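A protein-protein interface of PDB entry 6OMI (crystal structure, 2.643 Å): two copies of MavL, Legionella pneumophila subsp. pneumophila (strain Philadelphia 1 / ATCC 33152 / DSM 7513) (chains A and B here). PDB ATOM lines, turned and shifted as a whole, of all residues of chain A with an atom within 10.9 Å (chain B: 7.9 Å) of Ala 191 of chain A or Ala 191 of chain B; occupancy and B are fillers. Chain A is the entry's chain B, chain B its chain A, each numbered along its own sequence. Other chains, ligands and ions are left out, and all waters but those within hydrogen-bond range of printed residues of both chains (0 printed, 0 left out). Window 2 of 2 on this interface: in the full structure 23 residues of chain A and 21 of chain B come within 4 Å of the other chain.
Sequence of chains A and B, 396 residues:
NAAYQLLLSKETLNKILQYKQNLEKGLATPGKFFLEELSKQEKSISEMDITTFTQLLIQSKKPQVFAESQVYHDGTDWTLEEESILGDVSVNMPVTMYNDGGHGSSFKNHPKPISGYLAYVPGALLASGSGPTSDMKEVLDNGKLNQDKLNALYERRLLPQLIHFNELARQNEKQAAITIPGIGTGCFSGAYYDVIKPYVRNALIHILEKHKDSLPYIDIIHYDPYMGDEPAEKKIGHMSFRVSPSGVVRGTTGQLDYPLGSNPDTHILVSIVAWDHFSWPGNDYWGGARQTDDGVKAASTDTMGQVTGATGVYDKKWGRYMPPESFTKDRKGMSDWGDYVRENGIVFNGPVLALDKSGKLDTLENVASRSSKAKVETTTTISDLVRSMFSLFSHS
The backbone carbonyl oxygen (O) of Gly 190 of chain B sits close to the backbone carbonyl oxygen (O) of Gly 190 of chain A (3.1 Å). The side-chain hydroxyl (OH) of Tyr 193 of chain A lies within hydrogen-bond range of the backbone NH (N) of Ser 128 of chain B (3.4 Å). SG of Cys 187 of chain A sits at hydrogen-bond distance from SG of Cys 187 of chain B, at 3.4 Å.
The side-chain hydroxyl of Ser 189 of chain A lies close to the backbone NH of Tyr 193 of chain A (3.4 Å). The backbone NH (N) of Tyr 193 of chain B sits close to the side-chain hydroxyl (OG) of Ser 189 of chain B, at 3.3 Å. The backbone carbonyl oxygen (O) of Phe 188 of chain A lies within hydrogen-bond range of the backbone NH (N) of Leu 126 of chain A (2.8 Å).
Tyr 193 of chain B touches Leu 126 of chain A (OH to O, 3.7 Å). CA of Ala 127 of chain A touches OH of Tyr 193 of chain B, 3.3 Å away. Ser 128 of chain A touches Tyr 193 of chain B (O to CE2, 3.6 Å). CE1 of Tyr 193 of chain B touches CA of Gly 190 of chain A (3.8 Å). Ala 191 of chain A touches Ala 191 of chain B (CB to CB, 3.6 Å). N of Ala 191 of chain A touches CE1 of Tyr 193 of chain B, at 3.9 Å. Tyr 193 of chain A touches Ala 127 of chain B (OH to CA, 3.3 Å). Gly 190 of chain B touches Tyr 193 of chain A.
Of chain B, only Ala 191 and Tyr 193 come within 4 Å of Ala 191 of chain A. Ala 191 of chain B touches just one residue of chain A: Ala 191. Gly 190 of chain A touches just these residues of chain B: Gly 190 (3.1 Å) and Tyr 193 (3.8 Å). Of chain A, only Gly 190 (3.1 Å) and Tyr 193 (3.7 Å) come within 4 Å of Gly 190 of chain B. Tyr 192 of chain B touches none of the printed residues of chain A. Of the printed residues of chain A, Ser 128 of chain B touches Tyr 193. Printed residues of chain A within 4 Å of Tyr 193 of chain B: Leu 126, Ala 127, Ser 128, Gly 190 and Ala 191. Phe 188 of chain B touches none of the printed residues of chain A. Thr 185 of chain A touches none of the printed residues of chain B. The nearest residue of chain B that does not touch Ala 191 of chain A is Gly 190 of chain B (4.1 Å).
Of the 28 printed residues of chain A, 7 touch a printed residue of chain B. Among the printed residues, 11 pairs touch across the chains. Among the printed residues, no Asp or Glu carboxylate lies within 4 Å of a Lys or Arg side-chain nitrogen of the other chain.
Ala 127 of chain A touches Tyr 193 of chain B, and with the chains exchanged Tyr 193 of chain A touches Ala 127 of chain B. Gly 190 of chain A touches its own counterpart, Gly 190 of chain B. Ala 191 of chain B touches its own counterpart, Ala 191 of chain A. Ala 191 of chain A touches Tyr 193 of chain B, but with the chains exchanged Tyr 193 of chain A does not touch Ala 191 of chain B (4.1 Å).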
ATOM      1  N   GLU A  68     -15.086 -14.018  16.083  1.00  0.00           N
ATOM      2  CA  GLU A  68     -15.562 -13.551  17.379  1.00  0.00           C
ATOM      3  C   GLU A  68     -14.699 -14.011  18.548  1.00  0.00           C
ATOM      4  O   GLU A  68     -15.026 -13.693  19.697  1.00  0.00           O
ATOM      5  CB  GLU A  68     -17.009 -14.013  17.604  1.00  0.00           C
ATOM      6  CG  GLU A  68     -17.944 -13.767  16.424  1.00  0.00           C
ATOM      7  CD  GLU A  68     -17.889 -14.873  15.381  1.00  0.00           C
ATOM      8  OE1 GLU A  68     -18.760 -14.891  14.484  1.00  0.00           O
ATOM      9  OE2 GLU A  68     -16.976 -15.723  15.455  1.00  0.00           O
ATOM     10  N   ALA A 124     -21.575  -6.023  11.586  1.00  0.00           N
ATOM     11  CA  ALA A 124     -20.830  -5.350  12.641  1.00  0.00           C
ATOM     12  C   ALA A 124     -20.297  -6.368  13.640  1.00  0.00           C
ATOM     13  O   ALA A 124     -21.062  -7.153  14.208  1.00  0.00           O
ATOM     14  CB  ALA A 124     -21.720  -4.327  13.342  1.00  0.00           C
ATOM     15  N   LEU A 125     -18.982  -6.359  13.846  1.00  0.00           N
ATOM     16  CA  LEU A 125     -18.328  -7.281  14.770  1.00  0.00           C
ATOM     17  C   LEU A 125     -18.283  -6.637  16.151  1.00  0.00           C
ATOM     18  O   LEU A 125     -17.493  -5.719  16.392  1.00  0.00           O
ATOM     19  CB  LEU A 125     -16.927  -7.632  14.278  1.00  0.00           C
ATOM     20  CG  LEU A 125     -16.205  -8.749  15.036  1.00  0.00           C
ATOM     21  CD1 LEU A 125     -16.887 -10.085  14.800  1.00  0.00           C
ATOM     22  CD2 LEU A 125     -14.742  -8.813  14.635  1.00  0.00           C
ATOM     23  N   LEU A 126     -19.134  -7.117  17.058  1.00  0.00           N
ATOM     24  CA  LEU A 126     -19.237  -6.572  18.406  1.00  0.00           C
ATOM     25  C   LEU A 126     -18.863  -7.610  19.460  1.00  0.00           C
ATOM     26  O   LEU A 126     -19.409  -7.608  20.565  1.00  0.00           O
ATOM     27  CB  LEU A 126     -20.643  -6.031  18.664  1.00  0.00           C
ATOM     28  CG  LEU A 126     -21.155  -4.986  17.672  1.00  0.00           C
ATOM     29  CD1 LEU A 126     -22.589  -4.595  17.996  1.00  0.00           C
ATOM     30  CD2 LEU A 126     -20.250  -3.763  17.668  1.00  0.00           C
ATOM     31  N   ALA A 127     -17.935  -8.505  19.128  1.00  0.00           N
ATOM     32  CA  ALA A 127     -17.495  -9.532  20.062  1.00  0.00           C
ATOM     33  C   ALA A 127     -16.093  -9.984  19.679  1.00  0.00           C
ATOM     34  O   ALA A 127     -15.785 -10.122  18.493  1.00  0.00           O
ATOM     35  CB  ALA A 127     -18.456 -10.725  20.076  1.00  0.00           C
ATOM     36  N   SER A 128     -15.253 -10.205  20.687  1.00  0.00           N
ATOM     37  CA  SER A 128     -13.904 -10.698  20.455  1.00  0.00           C
ATOM     38  C   SER A 128     -13.367 -11.318  21.735  1.00  0.00           C
ATOM     39  O   SER A 128     -13.683 -10.865  22.838  1.00  0.00           O
ATOM     40  CB  SER A 128     -12.968  -9.584  19.984  1.00  0.00           C
ATOM     41  OG  SER A 128     -12.471  -8.840  21.081  1.00  0.00           O
ATOM     42  N   GLY A 129     -12.547 -12.356  21.572  1.00  0.00           N
ATOM     43  CA  GLY A 129     -11.908 -12.992  22.707  1.00  0.00           C
ATOM     44  C   GLY A 129     -10.762 -12.214  23.312  1.00  0.00           C
ATOM     45  O   GLY A 129     -10.333 -12.533  24.424  1.00  0.00           O
ATOM     46  N   THR A 133     -12.716  -4.443  19.230  1.00  0.00           N
ATOM     47  CA  THR A 133     -12.573  -4.455  17.784  1.00  0.00           C
ATOM     48  C   THR A 133     -12.791  -3.053  17.223  1.00  0.00           C
ATOM     49  O   THR A 133     -13.166  -2.120  17.936  1.00  0.00           O
ATOM     50  CB  THR A 133     -13.563  -5.435  17.152  1.00  0.00           C
ATOM     51  OG1 THR A 133     -14.868  -4.844  17.124  1.00  0.00           O
ATOM     52  CG2 THR A 133     -13.623  -6.722  17.951  1.00  0.00           C
ATOM     53  N   MET A 136     -16.569  -2.115  17.215  1.00  0.00           N
ATOM     54  CA  MET A 136     -16.924  -1.734  18.576  1.00  0.00           C
ATOM     55  C   MET A 136     -16.477  -0.308  18.864  1.00  0.00           C
ATOM     56  O   MET A 136     -17.227   0.483  19.429  1.00  0.00           O
ATOM     57  CB  MET A 136     -16.303  -2.697  19.588  1.00  0.00           C
ATOM     58  CG  MET A 136     -16.890  -4.095  19.555  1.00  0.00           C
ATOM     59  SD  MET A 136     -16.083  -5.264  20.888  1.00  0.00           S
ATOM     60  CE  MET A 136     -16.471  -4.212  22.483  1.00  0.00           C
ATOM     61  N   LEU A 140     -20.008   2.161  19.186  1.00  0.00           N
ATOM     62  CA  LEU A 140     -20.289   2.133  20.615  1.00  0.00           C
ATOM     63  C   LEU A 140     -19.840   3.437  21.259  1.00  0.00           C
ATOM     64  O   LEU A 140     -18.741   3.932  20.987  1.00  0.00           O
ATOM     65  CB  LEU A 140     -19.607   0.950  21.306  1.00  0.00           C
ATOM     66  CG  LEU A 140     -20.079  -0.448  20.901  1.00  0.00           C
ATOM     67  CD1 LEU A 140     -19.290  -1.523  21.637  1.00  0.00           C
ATOM     68  CD2 LEU A 140     -21.568  -0.598  21.165  1.00  0.00           C
ATOM     69  N   GLY A 143     -20.206   2.015  25.972  1.00  0.00           N
ATOM     70  CA  GLY A 143     -20.958   0.788  26.142  1.00  0.00           C
ATOM     71  C   GLY A 143     -22.268   0.775  25.381  1.00  0.00           C
ATOM     72  O   GLY A 143     -22.736  -0.284  24.954  1.00  0.00           O
ATOM     73  N   LYS A 144     -22.866   1.949  25.201  1.00  0.00           N
ATOM     74  CA  LYS A 144     -24.145   2.053  24.516  1.00  0.00           C
ATOM     75  C   LYS A 144     -23.965   1.887  23.013  1.00  0.00           C
ATOM     76  O   LYS A 144     -22.946   2.279  22.439  1.00  0.00           O
ATOM     77  CB  LYS A 144     -24.805   3.400  24.816  1.00  0.00           C
ATOM     78  N   LEU A 145     -24.977   1.305  22.374  1.00  0.00           N
ATOM     79  CA  LEU A 145     -24.956   1.061  20.936  1.00  0.00           C
ATOM     80  C   LEU A 145     -25.616   2.245  20.237  1.00  0.00           C
ATOM     81  O   LEU A 145     -26.817   2.479  20.397  1.00  0.00           O
ATOM     82  CB  LEU A 145     -25.666  -0.250  20.606  1.00  0.00           C
ATOM     83  CG  LEU A 145     -25.674  -0.713  19.147  1.00  0.00           C
ATOM     84  CD1 LEU A 145     -24.255  -0.863  18.624  1.00  0.00           C
ATOM     85  CD2 LEU A 145     -26.440  -2.021  19.003  1.00  0.00           C
ATOM     86  N   GLY A 184     -25.263  -9.655  11.343  1.00  0.00           N
ATOM     87  CA  GLY A 184     -24.598  -9.176  12.541  1.00  0.00           C
ATOM     88  C   GLY A 184     -25.424  -9.334  13.796  1.00  0.00           C
ATOM     89  O   GLY A 184     -25.304  -8.522  14.719  1.00  0.00           O
ATOM     90  N   THR A 185     -26.255 -10.372  13.859  1.00  0.00           N
ATOM     91  CA  THR A 185     -27.164 -10.571  14.979  1.00  0.00           C
ATOM     92  C   THR A 185     -27.024 -11.934  15.638  1.00  0.00           C
ATOM     93  O   THR A 185     -27.433 -12.079  16.798  1.00  0.00           O
ATOM     94  CB  THR A 185     -28.624 -10.364  14.531  1.00  0.00           C
ATOM     95  OG1 THR A 185     -29.314  -9.568  15.500  1.00  0.00           O
ATOM     96  CG2 THR A 185     -29.359 -11.692  14.359  1.00  0.00           C
ATOM     97  N   GLY A 186     -26.441 -12.921  14.961  1.00  0.00           N
ATOM     98  CA  GLY A 186     -26.259 -14.241  15.524  1.00  0.00           C
ATOM     99  C   GLY A 186     -25.336 -14.205  16.722  1.00  0.00           C
ATOM    100  O   GLY A 186     -25.792 -14.229  17.868  1.00  0.00           O
ATOM    101  N   CYS A 187     -24.029 -14.146  16.467  1.00  0.00           N
ATOM    102  CA  CYS A 187     -23.053 -14.022  17.536  1.00  0.00           C
ATOM    103  C   CYS A 187     -22.035 -12.915  17.301  1.00  0.00           C
ATOM    104  O   CYS A 187     -21.165 -12.710  18.156  1.00  0.00           O
ATOM    105  CB  CYS A 187     -22.325 -15.356  17.741  1.00  0.00           C
ATOM    106  SG  CYS A 187     -23.410 -16.648  18.378  1.00  0.00           S
ATOM    107  N   PHE A 188     -22.116 -12.195  16.182  1.00  0.00           N
ATOM    108  CA  PHE A 188     -21.290 -11.016  15.958  1.00  0.00           C
ATOM    109  C   PHE A 188     -21.768  -9.808  16.755  1.00  0.00           C
ATOM    110  O   PHE A 188     -21.388  -8.675  16.439  1.00  0.00           O
ATOM    111  CB  PHE A 188     -21.248 -10.676  14.465  1.00  0.00           C
ATOM    112  N   SER A 189     -22.582 -10.031  17.786  1.00  0.00           N
ATOM    113  CA  SER A 189     -23.071  -8.967  18.647  1.00  0.00           C
ATOM    114  C   SER A 189     -22.612  -9.098  20.088  1.00  0.00           C
ATOM    115  O   SER A 189     -22.663  -8.105  20.822  1.00  0.00           O
ATOM    116  CB  SER A 189     -24.607  -8.917  18.620  1.00  0.00           C
ATOM    117  OG  SER A 189     -25.163 -10.161  19.007  1.00  0.00           O
ATOM    118  N   GLY A 190     -22.160 -10.279  20.509  1.00  0.00           N
ATOM    119  CA  GLY A 190     -21.642 -10.477  21.847  1.00  0.00           C
ATOM    120  C   GLY A 190     -22.613 -10.101  22.945  1.00  0.00           C
ATOM    121  O   GLY A 190     -23.572 -10.828  23.217  1.00  0.00           O
ATOM    122  N   ALA A 191     -22.369  -8.958  23.580  1.00  0.00           N
ATOM    123  CA  ALA A 191     -23.178  -8.479  24.690  1.00  0.00           C
ATOM    124  C   ALA A 191     -24.361  -7.634  24.237  1.00  0.00           C
ATOM    125  O   ALA A 191     -25.004  -6.990  25.073  1.00  0.00           O
ATOM    126  CB  ALA A 191     -22.310  -7.677  25.662  1.00  0.00           C
ATOM    127  N   TYR A 192     -24.666  -7.623  22.939  1.00  0.00           N
ATOM    128  CA  TYR A 192     -25.754  -6.816  22.397  1.00  0.00           C
ATOM    129  C   TYR A 192     -26.784  -7.659  21.658  1.00  0.00           C
ATOM    130  O   TYR A 192     -27.629  -7.101  20.949  1.00  0.00           O
ATOM    131  CB  TYR A 192     -25.199  -5.728  21.474  1.00  0.00           C
ATOM    132  CG  TYR A 192     -24.191  -4.823  22.147  1.00  0.00           C
ATOM    133  CD1 TYR A 192     -22.839  -5.140  22.156  1.00  0.00           C
ATOM    134  CD2 TYR A 192     -24.594  -3.654  22.779  1.00  0.00           C
ATOM    135  CE1 TYR A 192     -21.916  -4.318  22.774  1.00  0.00           C
ATOM    136  CE2 TYR A 192     -23.679  -2.825  23.399  1.00  0.00           C
ATOM    137  CZ  TYR A 192     -22.342  -3.161  23.394  1.00  0.00           C
ATOM    138  OH  TYR A 192     -21.427  -2.337  24.011  1.00  0.00           O
ATOM    139  N   TYR A 193     -26.736  -8.985  21.814  1.00  0.00           N
ATOM    140  CA  TYR A 193     -27.693  -9.869  21.153  1.00  0.00           C
ATOM    141  C   TYR A 193     -29.134  -9.507  21.489  1.00  0.00           C
ATOM    142  O   TYR A 193     -30.033  -9.711  20.665  1.00  0.00           O
ATOM    143  CB  TYR A 193     -27.420 -11.318  21.557  1.00  0.00           C
ATOM    144  CG  TYR A 193     -27.749 -11.604  23.007  1.00  0.00           C
ATOM    145  CD1 TYR A 193     -26.913 -11.175  24.032  1.00  0.00           C
ATOM    146  CD2 TYR A 193     -28.908 -12.288  23.351  1.00  0.00           C
ATOM    147  CE1 TYR A 193     -27.219 -11.428  25.357  1.00  0.00           C
ATOM    148  CE2 TYR A 193     -29.221 -12.546  24.672  1.00  0.00           C
ATOM    149  CZ  TYR A 193     -28.374 -12.114  25.671  1.00  0.00           C
ATOM    150  OH  TYR A 193     -28.687 -12.371  26.985  1.00  0.00           O
ATOM    151  N   ASP A 194     -29.374  -8.972  22.683  1.00  0.00           N
ATOM    152  CA  ASP A 194     -30.722  -8.723  23.174  1.00  0.00           C
ATOM    153  C   ASP A 194     -31.267  -7.358  22.775  1.00  0.00           C
ATOM    154  O   ASP A 194     -32.391  -7.021  23.163  1.00  0.00           O
ATOM    155  CB  ASP A 194     -30.758  -8.856  24.701  1.00  0.00           C
ATOM    156  CG  ASP A 194     -29.712  -7.996  25.389  1.00  0.00           C
ATOM    157  OD1 ASP A 194     -28.892  -7.369  24.684  1.00  0.00           O
ATOM    158  OD2 ASP A 194     -29.711  -7.945  26.637  1.00  0.00           O
ATOM    159  N   VAL A 195     -30.511  -6.568  22.014  1.00  0.00           N
ATOM    160  CA  VAL A 195     -30.937  -5.215  21.676  1.00  0.00           C
ATOM    161  C   VAL A 195     -30.636  -4.913  20.212  1.00  0.00           C
ATOM    162  O   VAL A 195     -31.136  -3.928  19.658  1.00  0.00           O
ATOM    163  CB  VAL A 195     -30.261  -4.188  22.606  1.00  0.00           C
ATOM    164  CG1 VAL A 195     -28.790  -4.024  22.242  1.00  0.00           C
ATOM    165  CG2 VAL A 195     -30.992  -2.849  22.576  1.00  0.00           C
ATOM    166  N   ILE A 196     -29.838  -5.767  19.565  1.00  0.00           N
ATOM    167  CA  ILE A 196     -29.313  -5.418  18.246  1.00  0.00           C
ATOM    168  C   ILE A 196     -30.275  -5.722  17.097  1.00  0.00           C
ATOM    169  O   ILE A 196     -30.114  -5.154  16.012  1.00  0.00           O
ATOM    170  CB  ILE A 196     -27.963  -6.118  18.004  1.00  0.00           C
ATOM    171  CG1 ILE A 196     -27.198  -5.451  16.856  1.00  0.00           C
ATOM    172  CG2 ILE A 196     -28.161  -7.603  17.741  1.00  0.00           C
ATOM    173  CD1 ILE A 196     -25.813  -6.008  16.637  1.00  0.00           C
ATOM    174  N   LYS A 197     -31.275  -6.586  17.285  1.00  0.00           N
ATOM    175  CA  LYS A 197     -32.194  -6.867  16.180  1.00  0.00           C
ATOM    176  C   LYS A 197     -33.029  -5.656  15.775  1.00  0.00           C
ATOM    177  O   LYS A 197     -33.118  -5.378  14.564  1.00  0.00           O
ATOM    178  CB  LYS A 197     -33.072  -8.082  16.500  1.00  0.00           C
ATOM    179  CG  LYS A 197     -32.296  -9.383  16.576  1.00  0.00           C
ATOM    180  CD  LYS A 197     -33.214 -10.573  16.773  1.00  0.00           C
ATOM    181  CE  LYS A 197     -32.452 -11.882  16.636  1.00  0.00           C
ATOM    182  NZ  LYS A 197     -33.352 -13.067  16.705  1.00  0.00           N
ATOM    183  N   TYR A 199     -32.183  -2.620  16.157  1.00  0.00           N
ATOM    184  CA  TYR A 199     -31.201  -1.698  15.595  1.00  0.00           C
ATOM    185  C   TYR A 199     -30.874  -2.054  14.150  1.00  0.00           C
ATOM    186  O   TYR A 199     -30.778  -1.170  13.292  1.00  0.00           O
ATOM    187  CB  TYR A 199     -29.933  -1.698  16.451  1.00  0.00           C
ATOM    188  CG  TYR A 199     -30.017  -0.825  17.685  1.00  0.00           C
ATOM    189  CD1 TYR A 199     -30.967  -1.067  18.667  1.00  0.00           C
ATOM    190  CD2 TYR A 199     -29.140   0.235  17.870  1.00  0.00           C
ATOM    191  CE1 TYR A 199     -31.045  -0.277  19.799  1.00  0.00           C
ATOM    192  CE2 TYR A 199     -29.212   1.033  18.997  1.00  0.00           C
ATOM    193  CZ  TYR A 199     -30.165   0.772  19.959  1.00  0.00           C
ATOM    194  OH  TYR A 199     -30.242   1.562  21.083  1.00  0.00           O
ATOM    195  N   LEU B 126     -26.869 -17.895  30.926  1.00  0.00           N
ATOM    196  CA  LEU B 126     -26.735 -16.458  31.130  1.00  0.00           C
ATOM    197  C   LEU B 126     -27.119 -15.679  29.876  1.00  0.00           C
ATOM    198  O   LEU B 126     -26.566 -14.611  29.605  1.00  0.00           O
ATOM    199  CB  LEU B 126     -25.316 -16.102  31.570  1.00  0.00           C
ATOM    200  CG  LEU B 126     -24.865 -16.677  32.915  1.00  0.00           C
ATOM    201  N   ALA B 127     -28.066 -16.206  29.103  1.00  0.00           N
ATOM    202  CA  ALA B 127     -28.526 -15.542  27.893  1.00  0.00           C
ATOM    203  C   ALA B 127     -29.934 -16.019  27.577  1.00  0.00           C
ATOM    204  O   ALA B 127     -30.238 -17.208  27.715  1.00  0.00           O
ATOM    205  CB  ALA B 127     -27.588 -15.817  26.712  1.00  0.00           C
ATOM    206  N   SER B 128     -30.787 -15.089  27.154  1.00  0.00           N
ATOM    207  CA  SER B 128     -32.148 -15.420  26.761  1.00  0.00           C
ATOM    208  C   SER B 128     -32.693 -14.305  25.885  1.00  0.00           C
ATOM    209  O   SER B 128     -32.349 -13.134  26.064  1.00  0.00           O
ATOM    210  CB  SER B 128     -33.055 -15.633  27.976  1.00  0.00           C
ATOM    211  OG  SER B 128     -33.540 -14.398  28.476  1.00  0.00           O
ATOM    212  N   MET B 136     -29.407 -16.564  35.771  1.00  0.00           N
ATOM    213  CA  MET B 136     -29.088 -15.142  35.815  1.00  0.00           C
ATOM    214  C   MET B 136     -29.565 -14.527  37.123  1.00  0.00           C
ATOM    215  O   MET B 136     -28.851 -13.749  37.749  1.00  0.00           O
ATOM    216  CB  MET B 136     -29.716 -14.408  34.628  1.00  0.00           C
ATOM    217  CG  MET B 136     -29.162 -14.817  33.276  1.00  0.00           C
ATOM    218  SD  MET B 136     -29.943 -13.794  31.811  1.00  0.00           S
ATOM    219  CE  MET B 136     -29.403 -12.007  32.375  1.00  0.00           C
ATOM    220  N   GLY B 143     -25.562  -7.039  37.579  1.00  0.00           N
ATOM    221  CA  GLY B 143     -24.767  -7.200  36.377  1.00  0.00           C
ATOM    222  C   GLY B 143     -23.484  -7.984  36.562  1.00  0.00           C
ATOM    223  O   GLY B 143     -23.028  -8.658  35.634  1.00  0.00           O
ATOM    224  N   CYS B 187     -21.685 -19.828  23.573  1.00  0.00           N
ATOM    225  CA  CYS B 187     -22.567 -18.697  23.334  1.00  0.00           C
ATOM    226  C   CYS B 187     -23.757 -18.662  24.281  1.00  0.00           C
ATOM    227  O   CYS B 187     -24.573 -17.737  24.191  1.00  0.00           O
ATOM    228  CB  CYS B 187     -23.055 -18.705  21.879  1.00  0.00           C
ATOM    229  SG  CYS B 187     -21.722 -18.385  20.702  1.00  0.00           S
ATOM    230  N   PHE B 188     -23.881 -19.637  25.182  1.00  0.00           N
ATOM    231  CA  PHE B 188     -24.865 -19.629  26.255  1.00  0.00           C
ATOM    232  C   PHE B 188     -24.488 -18.679  27.388  1.00  0.00           C
ATOM    233  O   PHE B 188     -24.981 -18.835  28.511  1.00  0.00           O
ATOM    234  CB  PHE B 188     -25.060 -21.046  26.800  1.00  0.00           C
ATOM    235  N   SER B 189     -23.621 -17.706  27.108  1.00  0.00           N
ATOM    236  CA  SER B 189     -23.173 -16.730  28.087  1.00  0.00           C
ATOM    237  C   SER B 189     -23.595 -15.304  27.771  1.00  0.00           C
ATOM    238  O   SER B 189     -23.542 -14.455  28.668  1.00  0.00           O
ATOM    239  CB  SER B 189     -21.642 -16.770  28.215  1.00  0.00           C
ATOM    240  OG  SER B 189     -21.031 -16.551  26.955  1.00  0.00           O
ATOM    241  N   GLY B 190     -24.008 -15.017  26.538  1.00  0.00           N
ATOM    242  CA  GLY B 190     -24.477 -13.698  26.167  1.00  0.00           C
ATOM    243  C   GLY B 190     -23.473 -12.589  26.407  1.00  0.00           C
ATOM    244  O   GLY B 190     -22.504 -12.447  25.655  1.00  0.00           O
ATOM    245  N   ALA B 191     -23.697 -11.796  27.450  1.00  0.00           N
ATOM    246  CA  ALA B 191     -22.842 -10.661  27.767  1.00  0.00           C
ATOM    247  C   ALA B 191     -21.677 -11.029  28.678  1.00  0.00           C
ATOM    248  O   ALA B 191     -20.995 -10.131  29.181  1.00  0.00           O
ATOM    249  CB  ALA B 191     -23.669  -9.547  28.415  1.00  0.00           C
ATOM    250  N   TYR B 192     -21.431 -12.321  28.899  1.00  0.00           N
ATOM    251  CA  TYR B 192     -20.370 -12.760  29.797  1.00  0.00           C
ATOM    252  C   TYR B 192     -19.374 -13.691  29.119  1.00  0.00           C
ATOM    253  O   TYR B 192     -18.560 -14.317  29.807  1.00  0.00           O
ATOM    254  CB  TYR B 192     -20.977 -13.429  31.032  1.00  0.00           C
ATOM    255  CG  TYR B 192     -21.954 -12.533  31.757  1.00  0.00           C
ATOM    256  CD1 TYR B 192     -21.510 -11.574  32.658  1.00  0.00           C
ATOM    257  CD2 TYR B 192     -23.320 -12.632  31.526  1.00  0.00           C
ATOM    258  CE1 TYR B 192     -22.399 -10.746  33.316  1.00  0.00           C
ATOM    259  CE2 TYR B 192     -24.217 -11.808  32.180  1.00  0.00           C
ATOM    260  CZ  TYR B 192     -23.750 -10.867  33.074  1.00  0.00           C
ATOM    261  OH  TYR B 192     -24.637 -10.044  33.728  1.00  0.00           O
ATOM    262  N   TYR B 193     -19.419 -13.794  27.788  1.00  0.00           N
ATOM    263  CA  TYR B 193     -18.485 -14.642  27.053  1.00  0.00           C
ATOM    264  C   TYR B 193     -17.032 -14.282  27.335  1.00  0.00           C
ATOM    265  O   TYR B 193     -16.157 -15.155  27.294  1.00  0.00           O
ATOM    266  CB  TYR B 193     -18.778 -14.546  25.554  1.00  0.00           C
ATOM    267  CG  TYR B 193     -18.487 -13.181  24.964  1.00  0.00           C
ATOM    268  CD1 TYR B 193     -19.349 -12.113  25.183  1.00  0.00           C
ATOM    269  CD2 TYR B 193     -17.355 -12.960  24.193  1.00  0.00           C
ATOM    270  CE1 TYR B 193     -19.093 -10.864  24.652  1.00  0.00           C
ATOM    271  CE2 TYR B 193     -17.090 -11.712  23.655  1.00  0.00           C
ATOM    272  CZ  TYR B 193     -17.963 -10.669  23.888  1.00  0.00           C
ATOM    273  OH  TYR B 193     -17.705  -9.427  23.356  1.00  0.00           O
ATOM    274  N   ASP B 194     -16.755 -13.014  27.625  1.00  0.00           N
ATOM    275  CA  ASP B 194     -15.393 -12.524  27.781  1.00  0.00           C
ATOM    276  C   ASP B 194     -14.860 -12.656  29.202  1.00  0.00           C
ATOM    277  O   ASP B 194     -13.721 -12.248  29.457  1.00  0.00           O
ATOM    278  CB  ASP B 194     -15.317 -11.060  27.339  1.00  0.00           C
ATOM    279  CG  ASP B 194     -16.354 -10.190  28.025  1.00  0.00           C
ATOM    280  OD1 ASP B 194     -17.193 -10.736  28.772  1.00  0.00           O
ATOM    281  OD2 ASP B 194     -16.331  -8.959  27.816  1.00  0.00           O
ATOM    282  N   VAL B 195     -15.638 -13.213  30.129  1.00  0.00           N
ATOM    283  CA  VAL B 195     -15.219 -13.290  31.525  1.00  0.00           C
ATOM    284  C   VAL B 195     -15.546 -14.662  32.098  1.00  0.00           C
ATOM    285  O   VAL B 195     -15.060 -15.024  33.175  1.00  0.00           O
ATOM    286  CB  VAL B 195     -15.878 -12.184  32.371  1.00  0.00           C
ATOM    287  CG1 VAL B 195     -15.382 -10.806  31.951  1.00  0.00           C
ATOM    288  CG2 VAL B 195     -17.395 -12.268  32.268  1.00  0.00           C
ATOM    289  N   ILE B 196     -16.354 -15.445  31.381  1.00  0.00           N
ATOM    290  CA  ILE B 196     -16.875 -16.684  31.953  1.00  0.00           C
ATOM    291  C   ILE B 196     -15.876 -17.830  31.852  1.00  0.00           C
ATOM    292  O   ILE B 196     -16.014 -18.825  32.571  1.00  0.00           O
ATOM    293  CB  ILE B 196     -18.207 -17.065  31.281  1.00  0.00           C
ATOM    294  CG1 ILE B 196     -18.971 -18.099  32.116  1.00  0.00           C
ATOM    295  CG2 ILE B 196     -17.975 -17.563  29.863  1.00  0.00           C
ATOM    296  CD1 ILE B 196     -19.273 -17.640  33.524  1.00  0.00           C
